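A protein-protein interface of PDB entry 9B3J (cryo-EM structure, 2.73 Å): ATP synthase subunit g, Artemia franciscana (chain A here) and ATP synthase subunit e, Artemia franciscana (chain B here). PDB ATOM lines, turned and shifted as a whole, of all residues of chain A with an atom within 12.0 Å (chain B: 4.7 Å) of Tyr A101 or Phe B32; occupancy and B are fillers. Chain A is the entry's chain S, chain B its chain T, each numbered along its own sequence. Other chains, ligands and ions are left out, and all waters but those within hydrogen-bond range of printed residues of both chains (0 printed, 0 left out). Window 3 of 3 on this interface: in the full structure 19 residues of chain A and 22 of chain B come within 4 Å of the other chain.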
ATOM      1  N   ALA A  84     -11.571 -26.104 -25.030  1.00  0.00           N
ATOM      2  CA  ALA A  84     -11.852 -26.052 -23.596  1.00  0.00           C
ATOM      3  C   ALA A  84     -11.123 -24.896 -22.914  1.00  0.00           C
ATOM      4  O   ALA A  84     -11.635 -24.314 -21.947  1.00  0.00           O
ATOM      5  CB  ALA A  84     -11.480 -27.376 -22.938  1.00  0.00           C
ATOM      6  N   TRP A  86     -10.547 -22.026 -24.441  1.00  0.00           N
ATOM      7  CA  TRP A  86     -11.385 -20.883 -24.796  1.00  0.00           C
ATOM      8  C   TRP A  86     -12.610 -20.799 -23.901  1.00  0.00           C
ATOM      9  O   TRP A  86     -13.075 -19.699 -23.586  1.00  0.00           O
ATOM     10  CB  TRP A  86     -11.813 -20.961 -26.259  1.00  0.00           C
ATOM     11  CG  TRP A  86     -10.887 -20.253 -27.188  1.00  0.00           C
ATOM     12  CD1 TRP A  86      -9.683 -20.697 -27.635  1.00  0.00           C
ATOM     13  CD2 TRP A  86     -11.091 -18.972 -27.789  1.00  0.00           C
ATOM     14  NE1 TRP A  86      -9.119 -19.772 -28.476  1.00  0.00           N
ATOM     15  CE2 TRP A  86      -9.966 -18.703 -28.586  1.00  0.00           C
ATOM     16  CE3 TRP A  86     -12.114 -18.029 -27.732  1.00  0.00           C
ATOM     17  CZ2 TRP A  86      -9.835 -17.531 -29.318  1.00  0.00           C
ATOM     18  CZ3 TRP A  86     -11.981 -16.865 -28.459  1.00  0.00           C
ATOM     19  CH2 TRP A  86     -10.851 -16.626 -29.241  1.00  0.00           C
ATOM     20  N   PHE A  87     -13.136 -21.952 -23.487  1.00  0.00           N
ATOM     21  CA  PHE A  87     -14.240 -21.973 -22.528  1.00  0.00           C
ATOM     22  C   PHE A  87     -13.824 -21.380 -21.188  1.00  0.00           C
ATOM     23  O   PHE A  87     -14.590 -20.644 -20.558  1.00  0.00           O
ATOM     24  CB  PHE A  87     -14.743 -23.404 -22.352  1.00  0.00           C
ATOM     25  CG  PHE A  87     -15.476 -23.644 -21.067  1.00  0.00           C
ATOM     26  CD1 PHE A  87     -16.791 -23.258 -20.928  1.00  0.00           C
ATOM     27  CD2 PHE A  87     -14.862 -24.293 -20.010  1.00  0.00           C
ATOM     28  CE1 PHE A  87     -17.474 -23.487 -19.753  1.00  0.00           C
ATOM     29  CE2 PHE A  87     -15.539 -24.520 -18.832  1.00  0.00           C
ATOM     30  CZ  PHE A  87     -16.845 -24.117 -18.705  1.00  0.00           C
ATOM     31  N   PHE A  88     -12.615 -21.701 -20.730  1.00  0.00           N
ATOM     32  CA  PHE A  88     -12.156 -21.138 -19.459  1.00  0.00           C
ATOM     33  C   PHE A  88     -11.769 -19.670 -19.582  1.00  0.00           C
ATOM     34  O   PHE A  88     -11.864 -18.922 -18.602  1.00  0.00           O
ATOM     35  CB  PHE A  88     -10.987 -21.944 -18.910  1.00  0.00           C
ATOM     36  CG  PHE A  88     -11.405 -23.178 -18.185  1.00  0.00           C
ATOM     37  CD1 PHE A  88     -11.844 -23.105 -16.880  1.00  0.00           C
ATOM     38  CD2 PHE A  88     -11.366 -24.410 -18.809  1.00  0.00           C
ATOM     39  CE1 PHE A  88     -12.232 -24.239 -16.206  1.00  0.00           C
ATOM     40  CE2 PHE A  88     -11.753 -25.545 -18.144  1.00  0.00           C
ATOM     41  CZ  PHE A  88     -12.187 -25.461 -16.840  1.00  0.00           C
ATOM     42  N   VAL A  89     -11.323 -19.239 -20.762  1.00  0.00           N
ATOM     43  CA  VAL A  89     -11.125 -17.813 -21.003  1.00  0.00           C
ATOM     44  C   VAL A  89     -12.456 -17.082 -20.927  1.00  0.00           C
ATOM     45  O   VAL A  89     -12.562 -16.017 -20.309  1.00  0.00           O
ATOM     46  CB  VAL A  89     -10.424 -17.597 -22.357  1.00  0.00           C
ATOM     47  CG1 VAL A  89     -10.585 -16.169 -22.835  1.00  0.00           C
ATOM     48  CG2 VAL A  89      -8.957 -17.943 -22.241  1.00  0.00           C
ATOM     49  N   GLY A  90     -13.495 -17.654 -21.539  1.00  0.00           N
ATOM     50  CA  GLY A  90     -14.825 -17.083 -21.421  1.00  0.00           C
ATOM     51  C   GLY A  90     -15.349 -17.093 -20.002  1.00  0.00           C
ATOM     52  O   GLY A  90     -16.081 -16.189 -19.599  1.00  0.00           O
ATOM     53  N   GLU A  91     -14.979 -18.106 -19.223  1.00  0.00           N
ATOM     54  CA  GLU A  91     -15.326 -18.101 -17.808  1.00  0.00           C
ATOM     55  C   GLU A  91     -14.588 -16.999 -17.061  1.00  0.00           C
ATOM     56  O   GLU A  91     -15.140 -16.408 -16.128  1.00  0.00           O
ATOM     57  CB  GLU A  91     -15.032 -19.466 -17.202  1.00  0.00           C
ATOM     58  CG  GLU A  91     -15.591 -19.669 -15.819  1.00  0.00           C
ATOM     59  CD  GLU A  91     -15.665 -21.131 -15.448  1.00  0.00           C
ATOM     60  OE1 GLU A  91     -15.677 -21.977 -16.367  1.00  0.00           O
ATOM     61  OE2 GLU A  91     -15.710 -21.437 -14.238  1.00  0.00           O
ATOM     62  N   CYS A  92     -13.350 -16.706 -17.462  1.00  0.00           N
ATOM     63  CA  CYS A  92     -12.629 -15.577 -16.879  1.00  0.00           C
ATOM     64  C   CYS A  92     -13.274 -14.252 -17.262  1.00  0.00           C
ATOM     65  O   CYS A  92     -13.313 -13.317 -16.455  1.00  0.00           O
ATOM     66  CB  CYS A  92     -11.165 -15.597 -17.317  1.00  0.00           C
ATOM     67  SG  CYS A  92     -10.206 -16.956 -16.644  1.00  0.00           S
ATOM     68  N   ILE A  93     -13.753 -14.150 -18.502  1.00  0.00           N
ATOM     69  CA  ILE A  93     -14.457 -12.951 -18.951  1.00  0.00           C
ATOM     70  C   ILE A  93     -15.741 -12.763 -18.153  1.00  0.00           C
ATOM     71  O   ILE A  93     -16.044 -11.661 -17.678  1.00  0.00           O
ATOM     72  CB  ILE A  93     -14.734 -13.034 -20.464  1.00  0.00           C
ATOM     73  CG1 ILE A  93     -13.437 -12.867 -21.255  1.00  0.00           C
ATOM     74  CG2 ILE A  93     -15.757 -12.002 -20.891  1.00  0.00           C
ATOM     75  CD1 ILE A  93     -13.639 -12.804 -22.751  1.00  0.00           C
ATOM     76  N   GLY A  94     -16.500 -13.845 -17.972  1.00  0.00           N
ATOM     77  CA  GLY A  94     -17.752 -13.757 -17.238  1.00  0.00           C
ATOM     78  C   GLY A  94     -17.563 -13.446 -15.765  1.00  0.00           C
ATOM     79  O   GLY A  94     -18.381 -12.745 -15.163  1.00  0.00           O
ATOM     80  N   LYS A  95     -16.499 -13.966 -15.163  1.00  0.00           N
ATOM     81  CA  LYS A  95     -16.234 -13.707 -13.755  1.00  0.00           C
ATOM     82  C   LYS A  95     -15.385 -12.465 -13.526  1.00  0.00           C
ATOM     83  O   LYS A  95     -15.143 -12.102 -12.370  1.00  0.00           O
ATOM     84  CB  LYS A  95     -15.553 -14.919 -13.115  1.00  0.00           C
ATOM     85  CG  LYS A  95     -14.070 -15.059 -13.411  1.00  0.00           C
ATOM     86  CD  LYS A  95     -13.590 -16.459 -13.063  1.00  0.00           C
ATOM     87  CE  LYS A  95     -12.113 -16.639 -13.339  1.00  0.00           C
ATOM     88  NZ  LYS A  95     -11.683 -18.043 -13.102  1.00  0.00           N
ATOM     89  N   GLY A  96     -14.930 -11.807 -14.587  1.00  0.00           N
ATOM     90  CA  GLY A  96     -14.137 -10.607 -14.426  1.00  0.00           C
ATOM     91  C   GLY A  96     -12.653 -10.877 -14.296  1.00  0.00           C
ATOM     92  O   GLY A  96     -11.952 -11.035 -15.301  1.00  0.00           O
ATOM     93  N   SER A  97     -12.164 -10.917 -13.059  1.00  0.00           N
ATOM     94  CA  SER A  97     -10.744 -11.095 -12.803  1.00  0.00           C
ATOM     95  C   SER A  97     -10.294 -12.505 -13.172  1.00  0.00           C
ATOM     96  O   SER A  97     -11.087 -13.448 -13.233  1.00  0.00           O
ATOM     97  CB  SER A  97     -10.429 -10.812 -11.336  1.00  0.00           C
ATOM     98  OG  SER A  97     -11.211 -11.633 -10.488  1.00  0.00           O
ATOM     99  N   VAL A  98      -8.992 -12.638 -13.427  1.00  0.00           N
ATOM    100  CA  VAL A  98      -8.442 -13.915 -13.868  1.00  0.00           C
ATOM    101  C   VAL A  98      -8.157 -14.825 -12.682  1.00  0.00           C
ATOM    102  O   VAL A  98      -8.569 -15.989 -12.664  1.00  0.00           O
ATOM    103  CB  VAL A  98      -7.179 -13.689 -14.718  1.00  0.00           C
ATOM    104  CG1 VAL A  98      -7.553 -13.530 -16.177  1.00  0.00           C
ATOM    105  CG2 VAL A  98      -6.421 -12.463 -14.234  1.00  0.00           C
ATOM    106  N   ILE A  99      -7.462 -14.312 -11.671  1.00  0.00           N
ATOM    107  CA  ILE A  99      -7.013 -15.129 -10.547  1.00  0.00           C
ATOM    108  C   ILE A  99      -8.215 -15.363  -9.637  1.00  0.00           C
ATOM    109  O   ILE A  99      -8.552 -14.523  -8.803  1.00  0.00           O
ATOM    110  CB  ILE A  99      -5.852 -14.478  -9.796  1.00  0.00           C
ATOM    111  CG1 ILE A  99      -4.691 -14.214 -10.754  1.00  0.00           C
ATOM    112  CG2 ILE A  99      -5.391 -15.366  -8.658  1.00  0.00           C
ATOM    113  CD1 ILE A  99      -3.489 -13.599 -10.094  1.00  0.00           C
ATOM    114  N   GLY A 100      -8.867 -16.507  -9.802  1.00  0.00           N
ATOM    115  CA  GLY A 100      -9.956 -16.872  -8.928  1.00  0.00           C
ATOM    116  C   GLY A 100     -11.213 -16.061  -9.188  1.00  0.00           C
ATOM    117  O   GLY A 100     -11.349 -15.344 -10.178  1.00  0.00           O
ATOM    118  N   TYR A 101     -12.152 -16.196  -8.251  1.00  0.00           N
ATOM    119  CA  TYR A 101     -13.429 -15.502  -8.313  1.00  0.00           C
ATOM    120  C   TYR A 101     -13.452 -14.253  -7.444  1.00  0.00           C
ATOM    121  O   TYR A 101     -14.535 -13.793  -7.067  1.00  0.00           O
ATOM    122  CB  TYR A 101     -14.565 -16.446  -7.921  1.00  0.00           C
ATOM    123  CG  TYR A 101     -14.997 -17.353  -9.045  1.00  0.00           C
ATOM    124  CD1 TYR A 101     -15.856 -16.900 -10.031  1.00  0.00           C
ATOM    125  CD2 TYR A 101     -14.541 -18.658  -9.124  1.00  0.00           C
ATOM    126  CE1 TYR A 101     -16.254 -17.723 -11.065  1.00  0.00           C
ATOM    127  CE2 TYR A 101     -14.933 -19.489 -10.157  1.00  0.00           C
ATOM    128  CZ  TYR A 101     -15.788 -19.013 -11.126  1.00  0.00           C
ATOM    129  OH  TYR A 101     -16.187 -19.827 -12.160  1.00  0.00           O
ATOM    130  N   ARG A 102     -12.278 -13.713  -7.122  1.00  0.00           N
ATOM    131  CA  ARG A 102     -12.104 -12.472  -6.367  1.00  0.00           C
ATOM    132  C   ARG A 102     -12.816 -12.487  -5.019  1.00  0.00           C
ATOM    133  O   ARG A 102     -13.948 -12.021  -4.900  1.00  0.00           O
ATOM    134  CB  ARG A 102     -12.577 -11.277  -7.195  1.00  0.00           C
ATOM    135  CG  ARG A 102     -11.704 -10.048  -7.044  1.00  0.00           C
ATOM    136  CD  ARG A 102     -10.310 -10.290  -7.601  1.00  0.00           C
ATOM    137  NE  ARG A 102      -9.420  -9.163  -7.349  1.00  0.00           N
ATOM    138  CZ  ARG A 102      -9.248  -8.143  -8.179  1.00  0.00           C
ATOM    139  NH1 ARG A 102      -9.886  -8.077  -9.334  1.00  0.00           N
ATOM    140  NH2 ARG A 102      -8.415  -7.163  -7.839  1.00  0.00           N
ATOM    141  N   GLY B  28     -19.706 -18.619 -15.887  1.00  0.00           N
ATOM    142  CA  GLY B  28     -18.965 -17.794 -14.954  1.00  0.00           C
ATOM    143  C   GLY B  28     -19.850 -16.797 -14.237  1.00  0.00           C
ATOM    144  O   GLY B  28     -19.689 -16.565 -13.034  1.00  0.00           O
ATOM    145  N   SER B  29     -20.811 -16.209 -14.960  1.00  0.00           N
ATOM    146  CA  SER B  29     -21.761 -15.299 -14.327  1.00  0.00           C
ATOM    147  C   SER B  29     -22.645 -16.027 -13.321  1.00  0.00           C
ATOM    148  O   SER B  29     -22.889 -15.522 -12.215  1.00  0.00           O
ATOM    149  CB  SER B  29     -22.616 -14.616 -15.390  1.00  0.00           C
ATOM    150  OG  SER B  29     -21.809 -13.902 -16.307  1.00  0.00           O
ATOM    151  N   TYR B  30     -23.120 -17.224 -13.682  1.00  0.00           N
ATOM    152  CA  TYR B  30     -23.977 -17.986 -12.783  1.00  0.00           C
ATOM    153  C   TYR B  30     -23.230 -18.438 -11.535  1.00  0.00           C
ATOM    154  O   TYR B  30     -23.765 -18.353 -10.424  1.00  0.00           O
ATOM    155  CB  TYR B  30     -24.563 -19.187 -13.520  1.00  0.00           C
ATOM    156  CG  TYR B  30     -25.180 -20.212 -12.604  1.00  0.00           C
ATOM    157  CD1 TYR B  30     -26.373 -19.951 -11.944  1.00  0.00           C
ATOM    158  CD2 TYR B  30     -24.573 -21.444 -12.403  1.00  0.00           C
ATOM    159  CE1 TYR B  30     -26.944 -20.887 -11.105  1.00  0.00           C
ATOM    160  CE2 TYR B  30     -25.135 -22.388 -11.567  1.00  0.00           C
ATOM    161  CZ  TYR B  30     -26.320 -22.104 -10.920  1.00  0.00           C
ATOM    162  OH  TYR B  30     -26.885 -23.042 -10.087  1.00  0.00           O
ATOM    163  N   ARG B  31     -21.990 -18.916 -11.691  1.00  0.00           N
ATOM    164  CA  ARG B  31     -21.249 -19.406 -10.534  1.00  0.00           C
ATOM    165  C   ARG B  31     -20.808 -18.262  -9.633  1.00  0.00           C
ATOM    166  O   ARG B  31     -20.800 -18.410  -8.408  1.00  0.00           O
ATOM    167  CB  ARG B  31     -20.044 -20.234 -10.981  1.00  0.00           C
ATOM    168  CG  ARG B  31     -19.337 -20.976  -9.847  1.00  0.00           C
ATOM    169  CD  ARG B  31     -18.200 -21.839 -10.376  1.00  0.00           C
ATOM    170  NE  ARG B  31     -17.378 -22.402  -9.310  1.00  0.00           N
ATOM    171  CZ  ARG B  31     -16.259 -23.086  -9.508  1.00  0.00           C
ATOM    172  NH1 ARG B  31     -15.794 -23.315 -10.725  1.00  0.00           N
ATOM    173  NH2 ARG B  31     -15.586 -23.548  -8.459  1.00  0.00           N
ATOM    174  N   PHE B  32     -20.435 -17.116 -10.215  1.00  0.00           N
ATOM    175  CA  PHE B  32     -20.076 -15.958  -9.403  1.00  0.00           C
ATOM    176  C   PHE B  32     -21.273 -15.435  -8.622  1.00  0.00           C
ATOM    177  O   PHE B  32     -21.143 -15.076  -7.442  1.00  0.00           O
ATOM    178  CB  PHE B  32     -19.499 -14.861 -10.290  1.00  0.00           C
ATOM    179  CG  PHE B  32     -19.004 -13.670  -9.532  1.00  0.00           C
ATOM    180  CD1 PHE B  32     -17.754 -13.683  -8.946  1.00  0.00           C
ATOM    181  CD2 PHE B  32     -19.782 -12.531  -9.414  1.00  0.00           C
ATOM    182  CE1 PHE B  32     -17.289 -12.589  -8.251  1.00  0.00           C
ATOM    183  CE2 PHE B  32     -19.322 -11.433  -8.719  1.00  0.00           C
ATOM    184  CZ  PHE B  32     -18.073 -11.463  -8.138  1.00  0.00           C
ATOM    185  N   GLY B  33     -22.449 -15.390  -9.258  1.00  0.00           N
ATOM    186  CA  GLY B  33     -23.651 -15.023  -8.534  1.00  0.00           C
ATOM    187  C   GLY B  33     -24.025 -16.028  -7.465  1.00  0.00           C
ATOM    188  O   GLY B  33     -24.558 -15.653  -6.418  1.00  0.00           O
ATOM    189  N   SER B  34     -23.752 -17.309  -7.710  1.00  0.00           N
ATOM    190  CA  SER B  34     -24.047 -18.331  -6.714  1.00  0.00           C
ATOM    191  C   SER B  34     -23.113 -18.223  -5.516  1.00  0.00           C
ATOM    192  O   SER B  34     -23.560 -18.260  -4.365  1.00  0.00           O
ATOM    193  CB  SER B  34     -23.952 -19.718  -7.348  1.00  0.00           C
ATOM    194  OG  SER B  34     -24.186 -20.729  -6.387  1.00  0.00           O
ATOM    195  N   LEU B  35     -21.813 -18.080  -5.764  1.00  0.00           N
ATOM    196  CA  LEU B  35     -20.852 -18.074  -4.668  1.00  0.00           C
ATOM    197  C   LEU B  35     -20.790 -16.738  -3.949  1.00  0.00           C
ATOM    198  O   LEU B  35     -20.225 -16.679  -2.855  1.00  0.00           O
ATOM    199  CB  LEU B  35     -19.452 -18.465  -5.164  1.00  0.00           C
ATOM    200  CG  LEU B  35     -18.621 -17.568  -6.090  1.00  0.00           C
ATOM    201  CD1 LEU B  35     -17.679 -16.642  -5.325  1.00  0.00           C
ATOM    202  CD2 LEU B  35     -17.826 -18.433  -7.054  1.00  0.00           C
ATOM    203  N   GLN B  36     -21.333 -15.666  -4.537  1.00  0.00           N
ATOM    204  CA  GLN B  36     -21.361 -14.391  -3.830  1.00  0.00           C
ATOM    205  C   GLN B  36     -22.238 -14.466  -2.589  1.00  0.00           C
ATOM    206  O   GLN B  36     -21.863 -13.963  -1.525  1.00  0.00           O
ATOM    207  CB  GLN B  36     -21.842 -13.286  -4.767  1.00  0.00           C
ATOM    208  CG  GLN B  36     -21.861 -11.913  -4.131  1.00  0.00           C
ATOM    209  CD  GLN B  36     -20.511 -11.514  -3.573  1.00  0.00           C
ATOM    210  OE1 GLN B  36     -20.272 -11.602  -2.369  1.00  0.00           O
ATOM    211  NE2 GLN B  36     -19.620 -11.064  -4.447  1.00  0.00           N
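OE2 of Glu A91 is in salt-bridge range of NH1 of Arg B31 (3.98 Å).
Of the 9 printed residues of chain B, 5 touch a printed residue of chain A. Hydrophobic or aromatic side chains of chain B within 4 Å of the printed part of chain A: Phe B32 and Leu B35. Of the 18 printed residues of chain A, 3 touch a printed residue of chain B. Hydrophobic or aromatic side chains of chain A within 4 Å of the printed part of chain B: Tyr A101. Among the printed residues, 6 pairs touch across the chains.
Among the printed residues, pairs that only touch across the chains: Glu A91 with Gly B28 (3.96 Å), Gly A94 with Ser B29 (3.8 Å), Tyr A101 with Arg B31 (3.4 Å), Tyr A101 with Phe B32 (3.2 Å) and Tyr A101 with Leu B35 (3.6 Å).
Tyr A101 touches just these residues of chain B: Arg B31, Phe B32 and Leu B35. Of chain A, only Tyr A101 comes within 4 Å of Phe B32. Gly B28 touches one residue of chain A. Of the printed residues of chain A, Ser B29 touches Gly A94. No residue of chain A comes within 4 Å of Gly B33. No residue of chain A comes within 4 Å of Ser B34. Of the printed residues of chain A, Arg B31 touches Glu A91 and Tyr A101. Printed residues of chain B within 4 Å of Gly A94: Ser B29. Ala A84 touches none of the printed residues of chain B. The nearest printed residue of chain A that does not touch Arg B31 is Phe A88 (6.6 Å).
OH of Tyr A101 lies within hydrogen-bond range of OE2 of Glu A91 (2.7 Å).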
